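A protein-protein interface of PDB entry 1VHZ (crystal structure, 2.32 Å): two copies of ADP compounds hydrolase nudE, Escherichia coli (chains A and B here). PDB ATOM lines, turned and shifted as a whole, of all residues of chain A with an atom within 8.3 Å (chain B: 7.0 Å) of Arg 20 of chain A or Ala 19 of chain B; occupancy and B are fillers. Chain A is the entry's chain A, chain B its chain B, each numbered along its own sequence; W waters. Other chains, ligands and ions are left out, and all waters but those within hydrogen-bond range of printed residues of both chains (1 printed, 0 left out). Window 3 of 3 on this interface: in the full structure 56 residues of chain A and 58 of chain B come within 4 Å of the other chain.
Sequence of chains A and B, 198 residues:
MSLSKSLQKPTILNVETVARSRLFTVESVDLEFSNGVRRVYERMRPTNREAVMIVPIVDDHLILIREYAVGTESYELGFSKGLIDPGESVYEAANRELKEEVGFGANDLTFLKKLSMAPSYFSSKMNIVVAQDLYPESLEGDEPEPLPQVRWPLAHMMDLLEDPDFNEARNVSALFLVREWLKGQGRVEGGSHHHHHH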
ATOM      1  N   THR A  17     -18.864  17.211  14.394  1.00  0.00           N
ATOM      2  CA  THR A  17     -19.408  17.906  15.575  1.00  0.00           C
ATOM      3  C   THR A  17     -18.250  18.002  16.563  1.00  0.00           C
ATOM      4  O   THR A  17     -17.661  16.971  16.881  1.00  0.00           O
ATOM      5  CB  THR A  17     -20.589  17.149  16.163  1.00  0.00           C
ATOM      6  OG1 THR A  17     -21.669  17.221  15.223  1.00  0.00           O
ATOM      7  CG2 THR A  17     -21.040  17.727  17.498  1.00  0.00           C
ATOM      8  N   VAL A  18     -17.928  19.199  17.018  1.00  0.00           N
ATOM      9  CA  VAL A  18     -16.764  19.326  17.899  1.00  0.00           C
ATOM     10  C   VAL A  18     -17.092  19.868  19.264  1.00  0.00           C
ATOM     11  O   VAL A  18     -16.200  20.038  20.106  1.00  0.00           O
ATOM     12  CB  VAL A  18     -15.726  20.196  17.153  1.00  0.00           C
ATOM     13  CG1 VAL A  18     -16.023  21.676  17.297  1.00  0.00           C
ATOM     14  CG2 VAL A  18     -14.308  19.874  17.564  1.00  0.00           C
ATOM     15  N   ALA A  19     -18.361  20.181  19.505  1.00  0.00           N
ATOM     16  CA  ALA A  19     -18.791  20.715  20.792  1.00  0.00           C
ATOM     17  C   ALA A  19     -20.313  20.804  20.817  1.00  0.00           C
ATOM     18  O   ALA A  19     -20.948  21.206  19.844  1.00  0.00           O
ATOM     19  CB  ALA A  19     -18.132  22.040  21.103  1.00  0.00           C
ATOM     20  N   ARG A  20     -20.898  20.352  21.924  1.00  0.00           N
ATOM     21  CA  ARG A  20     -22.353  20.366  22.028  1.00  0.00           C
ATOM     22  C   ARG A  20     -22.821  20.690  23.437  1.00  0.00           C
ATOM     23  O   ARG A  20     -22.355  20.124  24.417  1.00  0.00           O
ATOM     24  CB  ARG A  20     -22.927  19.053  21.505  1.00  0.00           C
ATOM     25  CG  ARG A  20     -22.571  17.813  22.263  1.00  0.00           C
ATOM     26  CD  ARG A  20     -22.084  16.658  21.431  1.00  0.00           C
ATOM     27  NE  ARG A  20     -22.829  16.326  20.249  1.00  0.00           N
ATOM     28  CZ  ARG A  20     -24.121  16.104  20.099  1.00  0.00           C
ATOM     29  NH1 ARG A  20     -24.954  16.177  21.130  1.00  0.00           N
ATOM     30  NH2 ARG A  20     -24.597  15.806  18.894  1.00  0.00           N
ATOM     31  N   SER A  21     -23.681  21.702  23.524  1.00  0.00           N
ATOM     32  CA  SER A  21     -24.263  22.120  24.795  1.00  0.00           C
ATOM     33  C   SER A  21     -25.738  21.705  24.716  1.00  0.00           C
ATOM     34  O   SER A  21     -26.095  21.073  23.721  1.00  0.00           O
ATOM     35  CB  SER A  21     -24.149  23.610  25.053  1.00  0.00           C
ATOM     36  OG  SER A  21     -24.959  24.363  24.163  1.00  0.00           O
ATOM     37  N   ARG A  22     -26.560  22.147  25.649  1.00  0.00           N
ATOM     38  CA  ARG A  22     -27.974  21.777  25.615  1.00  0.00           C
ATOM     39  C   ARG A  22     -28.697  22.446  24.458  1.00  0.00           C
ATOM     40  O   ARG A  22     -29.600  21.853  23.865  1.00  0.00           O
ATOM     41  CB  ARG A  22     -28.651  22.076  26.953  1.00  0.00           C
ATOM     42  CG  ARG A  22     -29.947  21.308  27.182  1.00  0.00           C
ATOM     43  CD  ARG A  22     -30.326  21.302  28.663  1.00  0.00           C
ATOM     44  NE  ARG A  22     -30.377  22.666  29.186  1.00  0.00           N
ATOM     45  CZ  ARG A  22     -31.376  23.513  28.967  1.00  0.00           C
ATOM     46  NH1 ARG A  22     -32.422  23.146  28.237  1.00  0.00           N
ATOM     47  NH2 ARG A  22     -31.314  24.741  29.471  1.00  0.00           N
ATOM     48  N   LEU A  23     -28.267  23.638  24.066  1.00  0.00           N
ATOM     49  CA  LEU A  23     -28.908  24.373  22.979  1.00  0.00           C
ATOM     50  C   LEU A  23     -28.034  24.593  21.765  1.00  0.00           C
ATOM     51  O   LEU A  23     -28.516  25.024  20.703  1.00  0.00           O
ATOM     52  CB  LEU A  23     -29.372  25.717  23.564  1.00  0.00           C
ATOM     53  CG  LEU A  23     -29.951  26.775  22.644  1.00  0.00           C
ATOM     54  CD1 LEU A  23     -31.235  26.299  21.970  1.00  0.00           C
ATOM     55  CD2 LEU A  23     -30.208  28.075  23.396  1.00  0.00           C
ATOM     56  N   PHE A  24     -26.727  24.320  21.855  1.00  0.00           N
ATOM     57  CA  PHE A  24     -25.831  24.531  20.741  1.00  0.00           C
ATOM     58  C   PHE A  24     -25.027  23.323  20.294  1.00  0.00           C
ATOM     59  O   PHE A  24     -24.518  22.540  21.092  1.00  0.00           O
ATOM     60  CB  PHE A  24     -24.783  25.622  21.095  1.00  0.00           C
ATOM     61  CG  PHE A  24     -25.402  26.966  21.332  1.00  0.00           C
ATOM     62  CD1 PHE A  24     -25.759  27.780  20.268  1.00  0.00           C
ATOM     63  CD2 PHE A  24     -25.657  27.404  22.620  1.00  0.00           C
ATOM     64  CE1 PHE A  24     -26.333  29.017  20.494  1.00  0.00           C
ATOM     65  CE2 PHE A  24     -26.231  28.634  22.851  1.00  0.00           C
ATOM     66  CZ  PHE A  24     -26.571  29.445  21.788  1.00  0.00           C
ATOM     67  N   THR A  25     -24.864  23.209  18.967  1.00  0.00           N
ATOM     68  CA  THR A  25     -24.045  22.130  18.435  1.00  0.00           C
ATOM     69  C   THR A  25     -23.111  22.724  17.386  1.00  0.00           C
ATOM     70  O   THR A  25     -23.524  23.186  16.327  1.00  0.00           O
ATOM     71  CB  THR A  25     -24.753  20.854  18.026  1.00  0.00           C
ATOM     72  OG1 THR A  25     -24.099  20.249  16.888  1.00  0.00           O
ATOM     73  CG2 THR A  25     -26.221  21.006  17.761  1.00  0.00           C
ATOM     74  N   VAL A  26     -21.842  22.851  17.777  1.00  0.00           N
ATOM     75  CA  VAL A  26     -20.826  23.426  16.911  1.00  0.00           C
ATOM     76  C   VAL A  26     -20.062  22.375  16.123  1.00  0.00           C
ATOM     77  O   VAL A  26     -19.605  21.345  16.598  1.00  0.00           O
ATOM     78  CB  VAL A  26     -19.905  24.407  17.635  1.00  0.00           C
ATOM     79  CG1 VAL A  26     -19.742  24.045  19.099  1.00  0.00           C
ATOM     80  CG2 VAL A  26     -18.539  24.549  16.966  1.00  0.00           C
ATOM     81  N   GLU A  27     -19.982  22.647  14.815  1.00  0.00           N
ATOM     82  CA  GLU A  27     -19.324  21.814  13.847  1.00  0.00           C
ATOM     83  C   GLU A  27     -18.041  22.430  13.286  1.00  0.00           C
ATOM     84  O   GLU A  27     -17.935  23.641  13.126  1.00  0.00           O
ATOM     85  CB  GLU A  27     -20.244  21.617  12.615  1.00  0.00           C
ATOM     86  CG  GLU A  27     -21.435  20.737  12.924  1.00  0.00           C
ATOM     87  CD  GLU A  27     -22.344  20.577  11.736  1.00  0.00           C
ATOM     88  OE1 GLU A  27     -22.299  21.445  10.844  1.00  0.00           O
ATOM     89  OE2 GLU A  27     -23.080  19.576  11.683  1.00  0.00           O
ATOM     90  N   MET A  44     -22.384  26.749  13.504  1.00  0.00           N
ATOM     91  CA  MET A  44     -23.443  26.097  14.276  1.00  0.00           C
ATOM     92  C   MET A  44     -24.107  25.083  13.345  1.00  0.00           C
ATOM     93  O   MET A  44     -24.209  25.347  12.140  1.00  0.00           O
ATOM     94  CB  MET A  44     -24.423  27.111  14.841  1.00  0.00           C
ATOM     95  CG  MET A  44     -24.530  26.951  16.367  1.00  0.00           C
ATOM     96  SD  MET A  44     -23.037  27.519  17.176  1.00  0.00           S
ATOM     97  CE  MET A  44     -22.775  26.265  18.409  1.00  0.00           C
ATOM     98  N   ARG A  45     -24.428  23.906  13.851  1.00  0.00           N
ATOM     99  CA  ARG A  45     -25.053  22.888  13.024  1.00  0.00           C
ATOM    100  C   ARG A  45     -26.225  23.484  12.239  1.00  0.00           C
ATOM    101  O   ARG A  45     -27.105  24.113  12.801  1.00  0.00           O
ATOM    102  CB  ARG A  45     -25.535  21.705  13.865  1.00  0.00           C
ATOM    103  CG  ARG A  45     -26.048  20.540  13.038  1.00  0.00           C
ATOM    104  CD  ARG A  45     -26.036  19.240  13.834  1.00  0.00           C
ATOM    105  NE  ARG A  45     -25.988  18.078  12.953  1.00  0.00           N
ATOM    106  CZ  ARG A  45     -26.956  17.685  12.133  1.00  0.00           C
ATOM    107  NH1 ARG A  45     -28.098  18.361  12.058  1.00  0.00           N
ATOM    108  NH2 ARG A  45     -26.796  16.607  11.371  1.00  0.00           N
ATOM    109  N   GLU B  16     -21.591  28.929  34.228  1.00  0.00           N
ATOM    110  CA  GLU B  16     -20.632  27.830  34.038  1.00  0.00           C
ATOM    111  C   GLU B  16     -20.342  27.538  32.583  1.00  0.00           C
ATOM    112  O   GLU B  16     -21.222  27.560  31.731  1.00  0.00           O
ATOM    113  CB  GLU B  16     -21.230  26.640  34.772  1.00  0.00           C
ATOM    114  CG  GLU B  16     -20.694  25.260  34.524  1.00  0.00           C
ATOM    115  CD  GLU B  16     -21.436  24.251  35.408  1.00  0.00           C
ATOM    116  OE1 GLU B  16     -21.399  24.457  36.642  1.00  0.00           O
ATOM    117  OE2 GLU B  16     -22.046  23.324  34.851  1.00  0.00           O
ATOM    118  N   THR B  17     -19.057  27.347  32.267  1.00  0.00           N
ATOM    119  CA  THR B  17     -18.711  27.000  30.880  1.00  0.00           C
ATOM    120  C   THR B  17     -19.161  25.553  30.686  1.00  0.00           C
ATOM    121  O   THR B  17     -18.848  24.699  31.511  1.00  0.00           O
ATOM    122  CB  THR B  17     -17.243  27.196  30.547  1.00  0.00           C
ATOM    123  OG1 THR B  17     -16.937  28.587  30.763  1.00  0.00           O
ATOM    124  CG2 THR B  17     -16.968  26.844  29.094  1.00  0.00           C
ATOM    125  N   VAL B  18     -19.891  25.314  29.611  1.00  0.00           N
ATOM    126  CA  VAL B  18     -20.475  23.988  29.375  1.00  0.00           C
ATOM    127  C   VAL B  18     -20.092  23.388  28.057  1.00  0.00           C
ATOM    128  O   VAL B  18     -20.417  22.242  27.733  1.00  0.00           O
ATOM    129  CB  VAL B  18     -21.991  24.221  29.574  1.00  0.00           C
ATOM    130  CG1 VAL B  18     -22.755  24.366  28.279  1.00  0.00           C
ATOM    131  CG2 VAL B  18     -22.597  23.243  30.549  1.00  0.00           C
ATOM    132  N   ALA B  19     -19.361  24.134  27.228  1.00  0.00           N
ATOM    133  CA  ALA B  19     -18.892  23.666  25.940  1.00  0.00           C
ATOM    134  C   ALA B  19     -17.966  24.694  25.295  1.00  0.00           C
ATOM    135  O   ALA B  19     -18.190  25.899  25.374  1.00  0.00           O
ATOM    136  CB  ALA B  19     -20.013  23.282  25.004  1.00  0.00           C
ATOM    137  N   ARG B  20     -16.875  24.197  24.706  1.00  0.00           N
ATOM    138  CA  ARG B  20     -15.920  25.077  24.058  1.00  0.00           C
ATOM    139  C   ARG B  20     -15.352  24.479  22.780  1.00  0.00           C
ATOM    140  O   ARG B  20     -15.049  23.304  22.664  1.00  0.00           O
ATOM    141  CB  ARG B  20     -14.818  25.563  24.989  1.00  0.00           C
ATOM    142  CG  ARG B  20     -14.367  24.642  26.083  1.00  0.00           C
ATOM    143  CD  ARG B  20     -13.208  25.161  26.898  1.00  0.00           C
ATOM    144  NE  ARG B  20     -13.558  25.534  28.259  1.00  0.00           N
ATOM    145  CZ  ARG B  20     -13.537  26.769  28.744  1.00  0.00           C
ATOM    146  NH1 ARG B  20     -13.171  27.791  27.977  1.00  0.00           N
ATOM    147  NH2 ARG B  20     -13.874  26.992  30.008  1.00  0.00           N
ATOM    148  N   SER B  21     -15.302  25.328  21.762  1.00  0.00           N
ATOM    149  CA  SER B  21     -14.755  24.992  20.453  1.00  0.00           C
ATOM    150  C   SER B  21     -13.669  26.031  20.165  1.00  0.00           C
ATOM    151  O   SER B  21     -13.534  26.989  20.931  1.00  0.00           O
ATOM    152  CB  SER B  21     -15.797  25.034  19.344  1.00  0.00           C
ATOM    153  OG  SER B  21     -16.121  26.393  19.034  1.00  0.00           O
ATOM    154  N   PHE B  24     -15.923  29.120  19.698  1.00  0.00           N
ATOM    155  CA  PHE B  24     -17.105  29.311  20.524  1.00  0.00           C
ATOM    156  C   PHE B  24     -16.961  28.791  21.950  1.00  0.00           C
ATOM    157  O   PHE B  24     -16.395  27.729  22.201  1.00  0.00           O
ATOM    158  CB  PHE B  24     -18.310  28.606  19.896  1.00  0.00           C
ATOM    159  CG  PHE B  24     -18.751  29.074  18.549  1.00  0.00           C
ATOM    160  CD1 PHE B  24     -19.652  30.118  18.409  1.00  0.00           C
ATOM    161  CD2 PHE B  24     -18.276  28.462  17.397  1.00  0.00           C
ATOM    162  CE1 PHE B  24     -20.060  30.548  17.158  1.00  0.00           C
ATOM    163  CE2 PHE B  24     -18.681  28.884  16.143  1.00  0.00           C
ATOM    164  CZ  PHE B  24     -19.578  29.929  16.023  1.00  0.00           C
ATOM    165  N   THR B  25     -17.477  29.576  22.894  1.00  0.00           N
ATOM    166  CA  THR B  25     -17.484  29.178  24.299  1.00  0.00           C
ATOM    167  C   THR B  25     -18.876  29.451  24.857  1.00  0.00           C
ATOM    168  O   THR B  25     -19.354  30.573  24.976  1.00  0.00           O
ATOM    169  CB  THR B  25     -16.317  29.626  25.147  1.00  0.00           C
ATOM    170  OG1 THR B  25     -16.740  29.972  26.475  1.00  0.00           O
ATOM    171  CG2 THR B  25     -15.506  30.769  24.573  1.00  0.00           C
ATOM    172  N   VAL B  26     -19.634  28.370  25.044  1.00  0.00           N
ATOM    173  CA  VAL B  26     -21.000  28.453  25.548  1.00  0.00           C
ATOM    174  C   VAL B  26     -21.091  28.269  27.051  1.00  0.00           C
ATOM    175  O   VAL B  26     -20.498  27.390  27.666  1.00  0.00           O
ATOM    176  CB  VAL B  26     -21.970  27.547  24.782  1.00  0.00           C
ATOM    177  CG1 VAL B  26     -21.286  26.279  24.320  1.00  0.00           C
ATOM    178  CG2 VAL B  26     -23.249  27.220  25.548  1.00  0.00           C
ATOM    179  N   GLU B  27     -21.833  29.190  27.657  1.00  0.00           N
ATOM    180  CA  GLU B  27     -22.087  29.252  29.072  1.00  0.00           C
ATOM    181  C   GLU B  27     -23.547  28.926  29.426  1.00  0.00           C
ATOM    182  O   GLU B  27     -24.476  29.265  28.707  1.00  0.00           O
ATOM    183  CB  GLU B  27     -21.792  30.649  29.617  1.00  0.00           C
ATOM    184  CG  GLU B  27     -20.298  31.004  29.661  1.00  0.00           C
ATOM    185  CD  GLU B  27     -20.121  32.420  30.173  1.00  0.00           C
ATOM    186  OE1 GLU B  27     -21.113  33.192  30.118  1.00  0.00           O
ATOM    187  OE2 GLU B  27     -19.020  32.763  30.651  1.00  0.00           O
ATOM    188  N   SER B  28     -23.701  28.270  30.558  1.00  0.00           N
ATOM    189  CA  SER B  28     -25.002  27.895  31.110  1.00  0.00           C
ATOM    190  C   SER B  28     -25.225  28.883  32.254  1.00  0.00           C
ATOM    191  O   SER B  28     -24.273  29.133  33.010  1.00  0.00           O
ATOM    192  CB  SER B  28     -24.943  26.464  31.623  1.00  0.00           C
ATOM    193  OG  SER B  28     -26.224  25.956  31.902  1.00  0.00           O
ATOM    194  N   GLU B  42     -28.762  29.332  28.157  1.00  0.00           N
ATOM    195  CA  GLU B  42     -27.452  29.101  27.558  1.00  0.00           C
ATOM    196  C   GLU B  42     -27.098  30.297  26.684  1.00  0.00           C
ATOM    197  O   GLU B  42     -27.966  30.871  26.018  1.00  0.00           O
ATOM    198  CB  GLU B  42     -27.394  27.813  26.757  1.00  0.00           C
ATOM    199  CG  GLU B  42     -27.156  26.571  27.600  1.00  0.00           C
ATOM    200  CD  GLU B  42     -26.829  25.364  26.739  1.00  0.00           C
ATOM    201  OE1 GLU B  42     -26.519  24.303  27.317  1.00  0.00           O
ATOM    202  OE2 GLU B  42     -26.879  25.491  25.499  1.00  0.00           O
ATOM    203  N   MET B  44     -23.543  32.593  24.677  1.00  0.00           N
ATOM    204  CA  MET B  44     -22.171  32.659  24.180  1.00  0.00           C
ATOM    205  C   MET B  44     -21.396  33.518  25.167  1.00  0.00           C
ATOM    206  O   MET B  44     -21.949  34.551  25.575  1.00  0.00           O
ATOM    207  CB  MET B  44     -22.210  33.301  22.788  1.00  0.00           C
ATOM    208  CG  MET B  44     -21.360  32.538  21.783  1.00  0.00           C
ATOM    209  SD  MET B  44     -21.552  30.757  21.963  1.00  0.00           S
ATOM    210  CE  MET B  44     -22.928  30.458  20.851  1.00  0.00           C
HETATM  211  O   HOH W   1     -27.525  24.293  30.018  1.00  0.00           O
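The backbone NH (N) of Arg 22 of chain A sits at hydrogen-bond distance from the side-chain carboxylate (OE1) of Glu 42 of chain B (2.7 Å). The side-chain hydroxyl (OG) of Ser 21 of chain A sits at hydrogen-bond distance from the side-chain carboxylate (OE2) of Glu 42 of chain B (2.6 Å). The side-chain carboxylate (OE2) of Glu 42 of chain B lies within hydrogen-bond range of the backbone NH (N) of Leu 23 of chain A, at 2.7 Å.
The backbone NH (N) of Val 18 of chain B lies within hydrogen-bond range of the backbone carbonyl oxygen (O) of Val 26 of chain B (2.9 Å). O of Ala 19 of chain A sits at hydrogen-bond distance from N of Val 26 of chain A (2.8 Å). The backbone carbonyl oxygen of Ala 19 of chain B is in hydrogen-bond range of the backbone NH of Val 26 of chain B, at 2.9 Å. The backbone NH (N) of Leu 23 of chain A lies close to the side-chain hydroxyl (OG) of Ser 21 of chain A (3.4 Å). OG of Ser 21 of chain A lies within hydrogen-bond range of N of Phe 24 of chain A, 2.9 Å away. The backbone carbonyl oxygen of Val 26 of chain A lies within hydrogen-bond range of the backbone NH of Val 18 of chain A.
Among the printed residues, pairs that only touch across the chains: Val 18 of chain A with Ser 21 of chain B (3.9 Å), Ala 19 of chain A with Arg 20 of chain B (3.7 Å), Arg 20 of chain A with Ala 19 of chain B (3.98 Å), Ser 21 of chain A with Val 18 of chain B (3.6 Å), Ser 21 of chain A with Val 26 of chain B (3.6 Å), Phe 24 of chain A with Val 26 of chain B (3.8 Å), Phe 24 of chain A with Glu 42 of chain B (3.7 Å), Phe 24 of chain A with Met 44 of chain B (3.7 Å), Val 26 of chain A with Ser 21 of chain B (3.7 Å) and Val 26 of chain A with Phe 24 of chain B (3.9 Å).
Arg 20 of chain A touches just one residue of chain B: Ala 19. Of chain A, only Arg 20 (3.98 Å) comes within 4 Å of Ala 19 of chain B. Printed residues of chain A within 4 Å of Val 26 of chain B: Ser 21 (3.6 Å) and Phe 24 (3.8 Å). Printed residues of chain B within 4 Å of Ala 19 of chain A: Arg 20. Of the printed residues of chain B, Val 18 of chain A touches Ser 21 (3.9 Å). Of the printed residues of chain A, Phe 24 of chain B touches Val 26.
Of the 13 printed residues of chain A, 8 touch a printed residue of chain B. Hydrophobic or aromatic side chains of chain A that line the printed part of chain B: Val 18, Ala 19, Leu 23, Phe 24 and Val 26. Hydrophobic or aromatic side chains of chain B within 4 Å of the printed part of chain A: Val 18, Ala 19, Phe 24, Val 26 and Met 44. Among the printed residues, 13 pairs touch across the chains.
Val 18 of chain A touches Ser 21 of chain B, and with the chains exchanged Ser 21 of chain A touches Val 18 of chain B. Ala 19 of chain A touches Arg 20 of chain B, and with the chains exchanged Arg 20 of chain A touches Ala 19 of chain B. Ser 21 of chain A touches Val 26 of chain B, and with the chains exchanged Val 26 of chain A touches Ser 21 of chain B. Phe 24 of chain A touches Met 44 of chain B, but with the chains exchanged Met 44 of chain A does not touch Phe 24 of chain B (4.2 Å). Of the 13 pairs that touch across the chains among the printed residues, 8 have their exchanged pair printed and touching as well.
Water W1 lies within hydrogen-bond range of the side-chain hydroxyl (OG) of Ser 28 of chain B, the side-chain carboxylate (OE1) of Glu 42 of chain B and the guanidinium group (NE) of Arg 22 of chain A.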
